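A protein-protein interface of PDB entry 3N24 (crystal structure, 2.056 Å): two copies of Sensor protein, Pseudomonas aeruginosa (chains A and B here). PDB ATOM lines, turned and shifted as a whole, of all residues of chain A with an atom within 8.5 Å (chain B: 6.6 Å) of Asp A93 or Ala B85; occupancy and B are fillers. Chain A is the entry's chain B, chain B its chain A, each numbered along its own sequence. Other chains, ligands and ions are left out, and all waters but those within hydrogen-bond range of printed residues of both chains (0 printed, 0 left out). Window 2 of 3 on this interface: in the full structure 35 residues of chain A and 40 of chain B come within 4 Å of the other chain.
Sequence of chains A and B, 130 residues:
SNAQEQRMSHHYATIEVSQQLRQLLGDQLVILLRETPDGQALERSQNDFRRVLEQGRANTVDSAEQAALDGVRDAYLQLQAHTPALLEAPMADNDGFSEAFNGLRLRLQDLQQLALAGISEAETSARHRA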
ATOM      1  N   LEU A  33      11.034  25.227   1.783  1.00  0.00           N
ATOM      2  CA  LEU A  33      12.486  25.116   1.838  1.00  0.00           C
ATOM      3  C   LEU A  33      12.976  24.355   3.068  1.00  0.00           C
ATOM      4  O   LEU A  33      14.178  24.132   3.226  1.00  0.00           O
ATOM      5  CB  LEU A  33      13.110  26.506   1.863  1.00  0.00           C
ATOM      6  CG  LEU A  33      12.940  27.374   0.626  1.00  0.00           C
ATOM      7  CD1 LEU A  33      13.406  28.792   0.925  1.00  0.00           C
ATOM      8  CD2 LEU A  33      13.742  26.761  -0.493  1.00  0.00           C
ATOM      9  N   ARG A  34      12.057  23.984   3.946  1.00  0.00           N
ATOM     10  CA  ARG A  34      12.424  23.257   5.165  1.00  0.00           C
ATOM     11  C   ARG A  34      12.657  21.764   4.907  1.00  0.00           C
ATOM     12  O   ARG A  34      12.208  21.226   3.895  1.00  0.00           O
ATOM     13  CB  ARG A  34      11.357  23.459   6.246  1.00  0.00           C
ATOM     14  CG  ARG A  34      11.506  24.759   7.026  1.00  0.00           C
ATOM     15  CD  ARG A  34      10.174  25.227   7.586  1.00  0.00           C
ATOM     16  NE  ARG A  34       9.247  24.115   7.769  1.00  0.00           N
ATOM     17  CZ  ARG A  34       8.011  24.237   8.243  1.00  0.00           C
ATOM     18  NH1 ARG A  34       7.248  23.160   8.373  1.00  0.00           N
ATOM     19  NH2 ARG A  34       7.540  25.426   8.592  1.00  0.00           N
ATOM     20  N   GLU A  35      13.365  21.101   5.818  1.00  0.00           N
ATOM     21  CA  GLU A  35      13.599  19.666   5.694  1.00  0.00           C
ATOM     22  C   GLU A  35      12.269  18.925   5.587  1.00  0.00           C
ATOM     23  O   GLU A  35      12.048  18.155   4.650  1.00  0.00           O
ATOM     24  CB  GLU A  35      14.405  19.129   6.881  1.00  0.00           C
ATOM     25  CG  GLU A  35      15.843  19.639   6.975  1.00  0.00           C
ATOM     26  CD  GLU A  35      16.799  18.908   6.046  1.00  0.00           C
ATOM     27  OE1 GLU A  35      17.958  18.673   6.452  1.00  0.00           O
ATOM     28  OE2 GLU A  35      16.396  18.567   4.914  1.00  0.00           O
ATOM     29  N   ASP A  93      22.780  22.603   5.768  1.00  0.00           N
ATOM     30  CA  ASP A  93      21.440  22.440   6.320  1.00  0.00           C
ATOM     31  C   ASP A  93      20.373  22.946   5.351  1.00  0.00           C
ATOM     32  O   ASP A  93      20.511  24.022   4.765  1.00  0.00           O
ATOM     33  CB  ASP A  93      21.323  23.182   7.654  1.00  0.00           C
ATOM     34  CG  ASP A  93      20.124  22.732   8.473  1.00  0.00           C
ATOM     35  OD1 ASP A  93      19.347  21.884   7.982  1.00  0.00           O
ATOM     36  OD2 ASP A  93      19.961  23.223   9.613  1.00  0.00           O
ATOM     37  N   ASN A  94      19.317  22.156   5.183  1.00  0.00           N
ATOM     38  CA  ASN A  94      18.156  22.578   4.410  1.00  0.00           C
ATOM     39  C   ASN A  94      17.249  23.458   5.272  1.00  0.00           C
ATOM     40  O   ASN A  94      16.650  24.426   4.784  1.00  0.00           O
ATOM     41  CB  ASN A  94      17.387  21.359   3.884  1.00  0.00           C
ATOM     42  CG  ASN A  94      16.591  21.660   2.619  1.00  0.00           C
ATOM     43  OD1 ASN A  94      16.628  22.774   2.098  1.00  0.00           O
ATOM     44  ND2 ASN A  94      15.870  20.659   2.119  1.00  0.00           N
ATOM     45  N   ASP A  95      17.158  23.124   6.561  1.00  0.00           N
ATOM     46  CA  ASP A  95      16.411  23.954   7.502  1.00  0.00           C
ATOM     47  C   ASP A  95      17.202  25.200   7.836  1.00  0.00           C
ATOM     48  O   ASP A  95      16.640  26.199   8.275  1.00  0.00           O
ATOM     49  CB  ASP A  95      16.047  23.193   8.778  1.00  0.00           C
ATOM     50  CG  ASP A  95      14.550  23.013   8.934  1.00  0.00           C
ATOM     51  OD1 ASP A  95      13.898  23.881   9.558  1.00  0.00           O
ATOM     52  OD2 ASP A  95      14.025  22.005   8.420  1.00  0.00           O
ATOM     53  N   GLY A  96      18.515  25.131   7.622  1.00  0.00           N
ATOM     54  CA  GLY A  96      19.377  26.280   7.794  1.00  0.00           C
ATOM     55  C   GLY A  96      19.132  27.280   6.682  1.00  0.00           C
ATOM     56  O   GLY A  96      19.067  28.474   6.918  1.00  0.00           O
ATOM     57  N   PHE A  97      19.008  26.799   5.455  1.00  0.00           N
ATOM     58  CA  PHE A  97      18.778  27.709   4.339  1.00  0.00           C
ATOM     59  C   PHE A  97      17.435  28.404   4.512  1.00  0.00           C
ATOM     60  O   PHE A  97      17.343  29.622   4.386  1.00  0.00           O
ATOM     61  CB  PHE A  97      18.818  26.990   2.995  1.00  0.00           C
ATOM     62  CG  PHE A  97      18.577  27.910   1.828  1.00  0.00           C
ATOM     63  CD1 PHE A  97      19.602  28.695   1.333  1.00  0.00           C
ATOM     64  CD2 PHE A  97      17.309  28.052   1.289  1.00  0.00           C
ATOM     65  CE1 PHE A  97      19.382  29.567   0.286  1.00  0.00           C
ATOM     66  CE2 PHE A  97      17.074  28.924   0.249  1.00  0.00           C
ATOM     67  CZ  PHE A  97      18.111  29.684  -0.262  1.00  0.00           C
ATOM     68  N   SER A  98      16.408  27.616   4.833  1.00  0.00           N
ATOM     69  CA  SER A  98      15.064  28.137   5.059  1.00  0.00           C
ATOM     70  C   SER A  98      15.076  29.295   6.036  1.00  0.00           C
ATOM     71  O   SER A  98      14.534  30.361   5.756  1.00  0.00           O
ATOM     72  CB  SER A  98      14.141  27.038   5.573  1.00  0.00           C
ATOM     73  OG  SER A  98      12.838  27.539   5.787  1.00  0.00           O
ATOM     74  N   GLU A  99      15.719  29.102   7.182  1.00  0.00           N
ATOM     75  CA  GLU A  99      15.721  30.145   8.198  1.00  0.00           C
ATOM     76  C   GLU A  99      16.517  31.381   7.773  1.00  0.00           C
ATOM     77  O   GLU A  99      16.167  32.498   8.143  1.00  0.00           O
ATOM     78  CB  GLU A  99      16.196  29.606   9.570  1.00  0.00           C
ATOM     79  CG  GLU A  99      17.707  29.524   9.755  1.00  0.00           C
ATOM     80  CD  GLU A  99      18.128  29.451  11.229  1.00  0.00           C
ATOM     81  OE1 GLU A  99      18.045  28.354  11.829  1.00  0.00           O
ATOM     82  OE2 GLU A  99      18.553  30.493  11.787  1.00  0.00           O
ATOM     83  N   ALA A 100      17.574  31.199   6.988  1.00  0.00           N
ATOM     84  CA  ALA A 100      18.366  32.350   6.551  1.00  0.00           C
ATOM     85  C   ALA A 100      17.613  33.143   5.482  1.00  0.00           C
ATOM     86  O   ALA A 100      17.615  34.368   5.467  1.00  0.00           O
ATOM     87  CB  ALA A 100      19.730  31.896   6.019  1.00  0.00           C
ATOM     88  N   ALA B  81      26.092  31.542   3.233  1.00  0.00           N
ATOM     89  CA  ALA B  81      26.765  30.519   4.028  1.00  0.00           C
ATOM     90  C   ALA B  81      25.970  29.201   4.078  1.00  0.00           C
ATOM     91  O   ALA B  81      26.544  28.120   4.263  1.00  0.00           O
ATOM     92  CB  ALA B  81      27.060  31.046   5.445  1.00  0.00           C
ATOM     93  N   HIS B  82      24.654  29.283   3.898  1.00  0.00           N
ATOM     94  CA  HIS B  82      23.802  28.086   3.945  1.00  0.00           C
ATOM     95  C   HIS B  82      23.352  27.579   2.588  1.00  0.00           C
ATOM     96  O   HIS B  82      22.489  26.719   2.503  1.00  0.00           O
ATOM     97  CB  HIS B  82      22.556  28.332   4.792  1.00  0.00           C
ATOM     98  CG  HIS B  82      22.822  28.377   6.264  1.00  0.00           C
ATOM     99  ND1 HIS B  82      23.054  29.554   6.941  1.00  0.00           N
ATOM    100  CD2 HIS B  82      22.868  27.393   7.193  1.00  0.00           C
ATOM    101  CE1 HIS B  82      23.242  29.294   8.221  1.00  0.00           C
ATOM    102  NE2 HIS B  82      23.133  27.990   8.402  1.00  0.00           N
ATOM    103  N   THR B  83      23.912  28.128   1.526  1.00  0.00           N
ATOM    104  CA  THR B  83      23.469  27.781   0.181  1.00  0.00           C
ATOM    105  C   THR B  83      24.139  26.515  -0.376  1.00  0.00           C
ATOM    106  O   THR B  83      23.474  25.694  -1.021  1.00  0.00           O
ATOM    107  CB  THR B  83      23.666  28.978  -0.777  1.00  0.00           C
ATOM    108  OG1 THR B  83      22.787  30.035  -0.389  1.00  0.00           O
ATOM    109  CG2 THR B  83      23.393  28.581  -2.220  1.00  0.00           C
ATOM    110  N   PRO B  84      25.453  26.352  -0.131  1.00  0.00           N
ATOM    111  CA  PRO B  84      26.186  25.180  -0.617  1.00  0.00           C
ATOM    112  C   PRO B  84      25.443  23.869  -0.380  1.00  0.00           C
ATOM    113  O   PRO B  84      25.505  22.975  -1.223  1.00  0.00           O
ATOM    114  CB  PRO B  84      27.470  25.224   0.204  1.00  0.00           C
ATOM    115  CG  PRO B  84      27.715  26.679   0.387  1.00  0.00           C
ATOM    116  CD  PRO B  84      26.349  27.298   0.562  1.00  0.00           C
ATOM    117  N   ALA B  85      24.763  23.752   0.753  1.00  0.00           N
ATOM    118  CA  ALA B  85      23.863  22.631   0.971  1.00  0.00           C
ATOM    119  C   ALA B  85      22.887  22.574  -0.198  1.00  0.00           C
ATOM    120  O   ALA B  85      22.950  21.659  -1.021  1.00  0.00           O
ATOM    121  CB  ALA B  85      23.116  22.795   2.284  1.00  0.00           C
ATOM    122  N   LEU B  86      21.997  23.569  -0.245  1.00  0.00           N
ATOM    123  CA  LEU B  86      21.047  23.807  -1.340  1.00  0.00           C
ATOM    124  C   LEU B  86      19.647  24.099  -0.794  1.00  0.00           C
ATOM    125  O   LEU B  86      19.322  25.238  -0.463  1.00  0.00           O
ATOM    126  CB  LEU B  86      20.998  22.646  -2.345  1.00  0.00           C
ATOM    127  CG  LEU B  86      21.461  22.923  -3.780  1.00  0.00           C
ATOM    128  CD1 LEU B  86      22.875  22.403  -4.011  1.00  0.00           C
ATOM    129  CD2 LEU B  86      20.501  22.303  -4.781  1.00  0.00           C
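The backbone NH (N) of Asp A95 is in hydrogen-bond range of the side-chain carboxylate (OD1) of Asp A93. The side-chain carboxylate (OD2) of Asp A93 lies close to the backbone NH (N) of Gly A96 (3.1 Å).
Among the printed residues, pairs that only touch across the chains: Phe A97 with Thr B83 (3.5 Å), Asp A93 with Ala B85 (3.5 Å), Phe A97 with Leu B86 (3.6 Å), Phe A97 with His B82 (3.7 Å) and Gly A96 with His B82 (3.7 Å).
Of the 11 printed residues of chain A, 3 touch a printed residue of chain B. Of the 6 printed residues of chain B, 4 touch a printed residue of chain A. Hydrophobic or aromatic side chains of chain B within 4 Å of the printed part of chain A: His B82 and Ala B85.
No position is printed for both chains. Of the 5 pairs that touch across the chains among the printed residues, none has its exchanged pair printed and touching as well.
Asp A93 touches just one residue of chain B: Ala B85 (3.5 Å). Of the printed residues of chain B, Phe A97 touches His B82 (3.7 Å), Thr B83 (3.5 Å) and Leu B86 (3.6 Å). Of the printed residues of chain A, Thr B83 touches Phe A97 (3.5 Å). Of the printed residues of chain B, Gly A96 touches His B82. Glu A99 touches none of the printed residues of chain B. The nearest residue of chain A that does not touch Ala B85 is Asn A94 (4.8 Å).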
